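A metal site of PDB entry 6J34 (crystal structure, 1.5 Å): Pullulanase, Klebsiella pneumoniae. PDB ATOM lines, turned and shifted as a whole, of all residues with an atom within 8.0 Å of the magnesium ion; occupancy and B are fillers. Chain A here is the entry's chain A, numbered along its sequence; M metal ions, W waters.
The magnesium ion is bound by OD1 of Asp 451 (2.1 Å). The magnesium ion is bound by water W1. Water W2 binds the magnesium ion (2.2 Å). OE2 of Glu 457 binds the magnesium ion, at 2.2 Å. OE2 of Glu 538 is bound to the magnesium ion. The magnesium ion is bound by the backbone carbonyl oxygen (O) of Leu 452 (2.3 Å). The magnesium ion has six donor atoms within binding distance.
OG of Ser 358 touches the magnesium ion (3.96 Å). Five residues have an atom within 4 Å of the magnesium ion: Ser 358, Asp 451, Leu 452, Glu 457 and Glu 538.
Water W1 bridges OE1 of Glu 538 (2.7 Å) and O of Val 455 (2.7 Å).
The side-chain carboxylate of Glu 457 is in salt-bridge range of the guanidinium group of Arg 550 (3.5 Å). The side-chain carboxylate (OE2) of Glu 457 sits close to the backbone NH (N) of Gly 539 (2.9 Å). O of Asp 451 is in hydrogen-bond range of N of Phe 532 (2.9 Å). OD2 of Asp 451 lies within hydrogen-bond range of ND1 of His 533 (2.9 Å). The side-chain carboxylate (OE1) of Glu 538 sits at hydrogen-bond distance from the side-chain hydroxyl (OG) of Ser 540, 2.6 Å away. OG of Ser 358 is in hydrogen-bond range of OD2 of Asp 451, 2.6 Å away. The backbone NH (N) of Asp 451 lies within hydrogen-bond range of the backbone carbonyl oxygen (O) of Val 536, at 2.9 Å. The side-chain carboxylate of Glu 457 lies within hydrogen-bond range of the backbone NH of Asn 357, at 2.8 Å.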
ATOM      1  N   LEU A 354      15.651 -33.125 -15.214  1.00  0.00           N
ATOM      2  CA  LEU A 354      15.475 -31.713 -15.534  1.00  0.00           C
ATOM      3  C   LEU A 354      14.636 -31.556 -16.790  1.00  0.00           C
ATOM      4  O   LEU A 354      14.567 -32.440 -17.640  1.00  0.00           O
ATOM      5  CB  LEU A 354      16.837 -31.031 -15.800  1.00  0.00           C
ATOM      6  CG  LEU A 354      17.779 -30.916 -14.592  1.00  0.00           C
ATOM      7  CD1 LEU A 354      19.214 -30.668 -15.096  1.00  0.00           C
ATOM      8  CD2 LEU A 354      17.320 -29.821 -13.612  1.00  0.00           C
ATOM      9  N   SER A 355      13.986 -30.398 -16.897  1.00  0.00           N
ATOM     10  CA  SER A 355      13.405 -29.968 -18.166  1.00  0.00           C
ATOM     11  C   SER A 355      14.506 -29.457 -19.088  1.00  0.00           C
ATOM     12  O   SER A 355      15.677 -29.354 -18.721  1.00  0.00           O
ATOM     13  CB  SER A 355      12.363 -28.882 -17.918  1.00  0.00           C
ATOM     14  OG  SER A 355      12.994 -27.685 -17.511  1.00  0.00           O
ATOM     15  N   THR A 356      14.113 -29.092 -20.311  1.00  0.00           N
ATOM     16  CA  THR A 356      15.071 -28.596 -21.298  1.00  0.00           C
ATOM     17  C   THR A 356      15.796 -27.372 -20.763  1.00  0.00           C
ATOM     18  O   THR A 356      15.189 -26.424 -20.257  1.00  0.00           O
ATOM     19  CB  THR A 356      14.345 -28.231 -22.602  1.00  0.00           C
ATOM     20  OG1 THR A 356      13.661 -29.374 -23.117  1.00  0.00           O
ATOM     21  CG2 THR A 356      15.366 -27.746 -23.640  1.00  0.00           C
ATOM     22  N   ASN A 357      17.126 -27.375 -20.892  1.00  0.00           N
ATOM     23  CA  ASN A 357      17.967 -26.261 -20.470  1.00  0.00           C
ATOM     24  C   ASN A 357      17.927 -26.035 -18.973  1.00  0.00           C
ATOM     25  O   ASN A 357      18.299 -24.950 -18.491  1.00  0.00           O
ATOM     26  CB  ASN A 357      17.653 -24.970 -21.251  1.00  0.00           C
ATOM     27  CG  ASN A 357      18.912 -24.151 -21.512  1.00  0.00           C
ATOM     28  OD1 ASN A 357      19.985 -24.705 -21.786  1.00  0.00           O
ATOM     29  ND2 ASN A 357      18.800 -22.829 -21.394  1.00  0.00           N
ATOM     30  N   SER A 358      17.518 -27.051 -18.211  1.00  0.00           N
ATOM     31  CA  SER A 358      17.657 -27.073 -16.752  1.00  0.00           C
ATOM     32  C   SER A 358      16.764 -26.062 -16.046  1.00  0.00           C
ATOM     33  O   SER A 358      17.058 -25.679 -14.905  1.00  0.00           O
ATOM     34  CB  SER A 358      19.119 -26.900 -16.313  1.00  0.00           C
ATOM     35  OG  SER A 358      20.014 -27.606 -17.164  1.00  0.00           O
ATOM     36  N   PHE A 450      27.763 -34.588 -16.957  1.00  0.00           N
ATOM     37  CA  PHE A 450      26.782 -34.005 -16.058  1.00  0.00           C
ATOM     38  C   PHE A 450      26.199 -32.749 -16.722  1.00  0.00           C
ATOM     39  O   PHE A 450      26.635 -32.336 -17.802  1.00  0.00           O
ATOM     40  CB  PHE A 450      27.415 -33.666 -14.712  1.00  0.00           C
ATOM     41  CG  PHE A 450      28.605 -32.772 -14.832  1.00  0.00           C
ATOM     42  CD1 PHE A 450      28.464 -31.394 -14.934  1.00  0.00           C
ATOM     43  CD2 PHE A 450      29.885 -33.309 -14.915  1.00  0.00           C
ATOM     44  CE1 PHE A 450      29.560 -30.568 -15.102  1.00  0.00           C
ATOM     45  CE2 PHE A 450      30.990 -32.490 -15.076  1.00  0.00           C
ATOM     46  CZ  PHE A 450      30.840 -31.114 -15.167  1.00  0.00           C
ATOM     47  N   ASP A 451      25.228 -32.108 -16.075  1.00  0.00           N
ATOM     48  CA  ASP A 451      24.524 -31.005 -16.720  1.00  0.00           C
ATOM     49  C   ASP A 451      25.396 -29.752 -16.699  1.00  0.00           C
ATOM     50  O   ASP A 451      25.526 -29.099 -15.666  1.00  0.00           O
ATOM     51  CB  ASP A 451      23.197 -30.728 -16.018  1.00  0.00           C
ATOM     52  CG  ASP A 451      22.493 -29.526 -16.599  1.00  0.00           C
ATOM     53  OD1 ASP A 451      22.618 -29.298 -17.835  1.00  0.00           O
ATOM     54  OD2 ASP A 451      21.845 -28.812 -15.821  1.00  0.00           O
ATOM     55  N   LEU A 452      25.987 -29.418 -17.842  1.00  0.00           N
ATOM     56  CA  LEU A 452      26.756 -28.197 -17.997  1.00  0.00           C
ATOM     57  C   LEU A 452      25.806 -27.045 -18.358  1.00  0.00           C
ATOM     58  O   LEU A 452      24.676 -27.251 -18.790  1.00  0.00           O
ATOM     59  CB  LEU A 452      27.855 -28.373 -19.054  1.00  0.00           C
ATOM     60  CG  LEU A 452      27.425 -28.896 -20.417  1.00  0.00           C
ATOM     61  CD1 LEU A 452      27.583 -27.813 -21.473  1.00  0.00           C
ATOM     62  CD2 LEU A 452      28.223 -30.133 -20.802  1.00  0.00           C
ATOM     63  N   ALA A 453      26.303 -25.824 -18.164  1.00  0.00           N
ATOM     64  CA  ALA A 453      25.472 -24.640 -18.383  1.00  0.00           C
ATOM     65  C   ALA A 453      25.682 -23.965 -19.733  1.00  0.00           C
ATOM     66  O   ALA A 453      24.795 -23.229 -20.177  1.00  0.00           O
ATOM     67  CB  ALA A 453      25.763 -23.583 -17.306  1.00  0.00           C
ATOM     68  N   THR A 454      26.814 -24.202 -20.404  1.00  0.00           N
ATOM     69  CA  THR A 454      27.314 -23.344 -21.464  1.00  0.00           C
ATOM     70  C   THR A 454      26.921 -23.799 -22.869  1.00  0.00           C
ATOM     71  O   THR A 454      27.511 -23.323 -23.847  1.00  0.00           O
ATOM     72  CB  THR A 454      28.831 -23.228 -21.348  1.00  0.00           C
ATOM     73  OG1 THR A 454      29.374 -24.520 -21.041  1.00  0.00           O
ATOM     74  CG2 THR A 454      29.164 -22.255 -20.236  1.00  0.00           C
ATOM     75  N   VAL A 455      25.953 -24.701 -23.000  1.00  0.00           N
ATOM     76  CA  VAL A 455      25.272 -24.972 -24.254  1.00  0.00           C
ATOM     77  C   VAL A 455      23.784 -24.762 -24.006  1.00  0.00           C
ATOM     78  O   VAL A 455      23.249 -25.218 -22.995  1.00  0.00           O
ATOM     79  CB  VAL A 455      25.560 -26.400 -24.766  1.00  0.00           C
ATOM     80  CG1 VAL A 455      24.724 -26.701 -26.002  1.00  0.00           C
ATOM     81  CG2 VAL A 455      27.052 -26.565 -25.080  1.00  0.00           C
ATOM     82  N   ASN A 456      23.120 -24.054 -24.914  1.00  0.00           N
ATOM     83  CA  ASN A 456      21.677 -23.873 -24.783  1.00  0.00           C
ATOM     84  C   ASN A 456      21.009 -25.147 -25.266  1.00  0.00           C
ATOM     85  O   ASN A 456      21.223 -25.575 -26.404  1.00  0.00           O
ATOM     86  CB  ASN A 456      21.212 -22.669 -25.600  1.00  0.00           C
ATOM     87  CG  ASN A 456      19.817 -22.235 -25.233  1.00  0.00           C
ATOM     88  OD1 ASN A 456      18.940 -23.062 -25.030  1.00  0.00           O
ATOM     89  ND2 ASN A 456      19.610 -20.929 -25.147  1.00  0.00           N
ATOM     90  N   GLU A 457      20.214 -25.769 -24.400  1.00  0.00           N
ATOM     91  CA  GLU A 457      19.591 -27.039 -24.744  1.00  0.00           C
ATOM     92  C   GLU A 457      18.316 -26.869 -25.567  1.00  0.00           C
ATOM     93  O   GLU A 457      17.760 -27.875 -26.031  1.00  0.00           O
ATOM     94  CB  GLU A 457      19.315 -27.866 -23.486  1.00  0.00           C
ATOM     95  CG  GLU A 457      20.593 -28.112 -22.681  1.00  0.00           C
ATOM     96  CD  GLU A 457      20.348 -28.987 -21.470  1.00  0.00           C
ATOM     97  OE1 GLU A 457      19.169 -29.268 -21.151  1.00  0.00           O
ATOM     98  OE2 GLU A 457      21.351 -29.398 -20.844  1.00  0.00           O
ATOM     99  N   ASP A 530      31.517 -26.423 -16.571  1.00  0.00           N
ATOM    100  CA  ASP A 530      30.626 -25.312 -16.241  1.00  0.00           C
ATOM    101  C   ASP A 530      29.397 -25.900 -15.552  1.00  0.00           C
ATOM    102  O   ASP A 530      28.323 -25.988 -16.136  1.00  0.00           O
ATOM    103  CB  ASP A 530      30.224 -24.583 -17.532  1.00  0.00           C
ATOM    104  CG  ASP A 530      31.413 -24.048 -18.294  1.00  0.00           C
ATOM    105  OD1 ASP A 530      32.191 -23.289 -17.675  1.00  0.00           O
ATOM    106  OD2 ASP A 530      31.551 -24.347 -19.501  1.00  0.00           O
ATOM    107  N   PRO A 531      29.547 -26.335 -14.300  1.00  0.00           N
ATOM    108  CA  PRO A 531      28.496 -27.179 -13.700  1.00  0.00           C
ATOM    109  C   PRO A 531      27.229 -26.391 -13.395  1.00  0.00           C
ATOM    110  O   PRO A 531      27.262 -25.374 -12.702  1.00  0.00           O
ATOM    111  CB  PRO A 531      29.148 -27.698 -12.409  1.00  0.00           C
ATOM    112  CG  PRO A 531      30.623 -27.486 -12.605  1.00  0.00           C
ATOM    113  CD  PRO A 531      30.765 -26.288 -13.477  1.00  0.00           C
ATOM    114  N   PHE A 532      26.114 -26.894 -13.915  1.00  0.00           N
ATOM    115  CA  PHE A 532      24.778 -26.380 -13.609  1.00  0.00           C
ATOM    116  C   PHE A 532      24.081 -27.273 -12.580  1.00  0.00           C
ATOM    117  O   PHE A 532      23.650 -26.780 -11.532  1.00  0.00           O
ATOM    118  CB  PHE A 532      23.990 -26.297 -14.925  1.00  0.00           C
ATOM    119  CG  PHE A 532      22.846 -25.306 -14.920  1.00  0.00           C
ATOM    120  CD1 PHE A 532      22.354 -24.778 -13.730  1.00  0.00           C
ATOM    121  CD2 PHE A 532      22.257 -24.934 -16.118  1.00  0.00           C
ATOM    122  CE1 PHE A 532      21.292 -23.875 -13.759  1.00  0.00           C
ATOM    123  CE2 PHE A 532      21.205 -24.034 -16.149  1.00  0.00           C
ATOM    124  CZ  PHE A 532      20.719 -23.518 -14.965  1.00  0.00           C
ATOM    125  N   HIS A 533      24.011 -28.587 -12.842  1.00  0.00           N
ATOM    126  CA  HIS A 533      23.538 -29.573 -11.883  1.00  0.00           C
ATOM    127  C   HIS A 533      24.494 -30.751 -11.887  1.00  0.00           C
ATOM    128  O   HIS A 533      24.822 -31.291 -12.948  1.00  0.00           O
ATOM    129  CB  HIS A 533      22.120 -30.041 -12.184  1.00  0.00           C
ATOM    130  CG  HIS A 533      21.119 -28.937 -12.118  1.00  0.00           C
ATOM    131  ND1 HIS A 533      20.936 -28.057 -13.159  1.00  0.00           N
ATOM    132  CD2 HIS A 533      20.315 -28.519 -11.112  1.00  0.00           C
ATOM    133  CE1 HIS A 533      20.029 -27.161 -12.818  1.00  0.00           C
ATOM    134  NE2 HIS A 533      19.644 -27.407 -11.571  1.00  0.00           N
ATOM    135  N   VAL A 536      22.647 -34.804 -12.821  1.00  0.00           N
ATOM    136  CA  VAL A 536      21.771 -35.086 -13.946  1.00  0.00           C
ATOM    137  C   VAL A 536      22.650 -35.120 -15.190  1.00  0.00           C
ATOM    138  O   VAL A 536      23.587 -34.326 -15.286  1.00  0.00           O
ATOM    139  CB  VAL A 536      20.707 -33.981 -14.129  1.00  0.00           C
ATOM    140  CG1 VAL A 536      19.673 -34.408 -15.151  1.00  0.00           C
ATOM    141  CG2 VAL A 536      20.059 -33.637 -12.811  1.00  0.00           C
ATOM    142  N   PRO A 537      22.400 -36.016 -16.148  1.00  0.00           N
ATOM    143  CA  PRO A 537      23.127 -35.948 -17.419  1.00  0.00           C
ATOM    144  C   PRO A 537      22.872 -34.639 -18.144  1.00  0.00           C
ATOM    145  O   PRO A 537      21.822 -34.012 -18.002  1.00  0.00           O
ATOM    146  CB  PRO A 537      22.553 -37.128 -18.224  1.00  0.00           C
ATOM    147  CG  PRO A 537      22.142 -38.114 -17.152  1.00  0.00           C
ATOM    148  CD  PRO A 537      21.571 -37.231 -16.047  1.00  0.00           C
ATOM    149  N   GLU A 538      23.860 -34.236 -18.954  1.00  0.00           N
ATOM    150  CA  GLU A 538      23.687 -33.081 -19.840  1.00  0.00           C
ATOM    151  C   GLU A 538      22.566 -33.325 -20.845  1.00  0.00           C
ATOM    152  O   GLU A 538      22.424 -34.429 -21.381  1.00  0.00           O
ATOM    153  CB  GLU A 538      25.024 -32.797 -20.563  1.00  0.00           C
ATOM    154  CG  GLU A 538      24.918 -31.906 -21.801  1.00  0.00           C
ATOM    155  CD  GLU A 538      24.377 -30.509 -21.533  1.00  0.00           C
ATOM    156  OE1 GLU A 538      24.120 -29.789 -22.512  1.00  0.00           O
ATOM    157  OE2 GLU A 538      24.209 -30.120 -20.358  1.00  0.00           O
ATOM    158  N   GLY A 539      21.747 -32.296 -21.077  1.00  0.00           N
ATOM    159  CA  GLY A 539      20.592 -32.448 -21.955  1.00  0.00           C
ATOM    160  C   GLY A 539      20.891 -32.344 -23.436  1.00  0.00           C
ATOM    161  O   GLY A 539      20.235 -32.994 -24.245  1.00  0.00           O
ATOM    162  N   SER A 540      21.893 -31.530 -23.826  1.00  0.00           N
ATOM    163  CA  SER A 540      22.110 -31.315 -25.248  1.00  0.00           C
ATOM    164  C   SER A 540      22.691 -32.543 -25.935  1.00  0.00           C
ATOM    165  O   SER A 540      22.610 -32.653 -27.168  1.00  0.00           O
ATOM    166  CB  SER A 540      23.024 -30.104 -25.476  1.00  0.00           C
ATOM    167  OG  SER A 540      24.355 -30.378 -25.069  1.00  0.00           O
ATOM    168  N   TYR A 541      23.265 -33.481 -25.182  1.00  0.00           N
ATOM    169  CA  TYR A 541      23.767 -34.725 -25.731  1.00  0.00           C
ATOM    170  C   TYR A 541      22.681 -35.782 -25.887  1.00  0.00           C
ATOM    171  O   TYR A 541      22.954 -36.870 -26.390  1.00  0.00           O
ATOM    172  CB  TYR A 541      24.923 -35.270 -24.880  1.00  0.00           C
ATOM    173  CG  TYR A 541      26.125 -34.354 -24.776  1.00  0.00           C
ATOM    174  CD1 TYR A 541      26.524 -33.572 -25.842  1.00  0.00           C
ATOM    175  CD2 TYR A 541      26.866 -34.287 -23.594  1.00  0.00           C
ATOM    176  CE1 TYR A 541      27.617 -32.724 -25.751  1.00  0.00           C
ATOM    177  CE2 TYR A 541      27.976 -33.455 -23.489  1.00  0.00           C
ATOM    178  CZ  TYR A 541      28.356 -32.684 -24.584  1.00  0.00           C
ATOM    179  OH  TYR A 541      29.432 -31.846 -24.509  1.00  0.00           O
ATOM    180  N   PRO A 545      15.908 -33.377 -24.903  1.00  0.00           N
ATOM    181  CA  PRO A 545      16.369 -32.850 -23.618  1.00  0.00           C
ATOM    182  C   PRO A 545      15.242 -32.567 -22.628  1.00  0.00           C
ATOM    183  O   PRO A 545      15.516 -32.097 -21.521  1.00  0.00           O
ATOM    184  CB  PRO A 545      17.040 -31.533 -24.039  1.00  0.00           C
ATOM    185  CG  PRO A 545      16.217 -31.080 -25.207  1.00  0.00           C
ATOM    186  CD  PRO A 545      15.897 -32.352 -25.968  1.00  0.00           C
ATOM    187  N   ARG A 550      16.782 -38.295 -21.416  1.00  0.00           N
ATOM    188  CA  ARG A 550      18.245 -38.336 -21.440  1.00  0.00           C
ATOM    189  C   ARG A 550      18.810 -39.417 -20.524  1.00  0.00           C
ATOM    190  O   ARG A 550      19.939 -39.886 -20.753  1.00  0.00           O
ATOM    191  CB  ARG A 550      18.830 -36.983 -21.041  1.00  0.00           C
ATOM    192  CG  ARG A 550      18.595 -36.623 -19.576  1.00  0.00           C
ATOM    193  CD  ARG A 550      19.132 -35.244 -19.255  1.00  0.00           C
ATOM    194  NE  ARG A 550      18.217 -34.184 -19.675  1.00  0.00           N
ATOM    195  CZ  ARG A 550      18.347 -32.917 -19.279  1.00  0.00           C
ATOM    196  NH1 ARG A 550      19.367 -32.580 -18.485  1.00  0.00           N
ATOM    197  NH2 ARG A 550      17.456 -31.996 -19.659  1.00  0.00           N
ATOM    198  N   ARG A 586      21.156 -16.796 -13.800  1.00  0.00           N
ATOM    199  CA  ARG A 586      20.315 -17.948 -14.151  1.00  0.00           C
ATOM    200  C   ARG A 586      20.895 -19.265 -13.643  1.00  0.00           C
ATOM    201  O   ARG A 586      20.144 -20.166 -13.240  1.00  0.00           O
ATOM    202  CB  ARG A 586      20.173 -17.996 -15.680  1.00  0.00           C
ATOM    203  CG  ARG A 586      19.671 -19.293 -16.275  1.00  0.00           C
ATOM    204  CD  ARG A 586      19.736 -19.291 -17.810  1.00  0.00           C
ATOM    205  NE  ARG A 586      21.096 -19.466 -18.323  1.00  0.00           N
ATOM    206  CZ  ARG A 586      21.601 -20.621 -18.769  1.00  0.00           C
ATOM    207  NH1 ARG A 586      20.857 -21.718 -18.775  1.00  0.00           N
ATOM    208  NH2 ARG A 586      22.852 -20.679 -19.210  1.00  0.00           N
HETATM  209 MG    MG M   1      22.953 -28.403 -19.701  1.00  0.00          MG
HETATM  210  O   HOH W   1      23.715 -27.370 -21.457  1.00  0.00           O
HETATM  211  O   HOH W   2      21.567 -26.752 -19.248  1.00  0.00           O
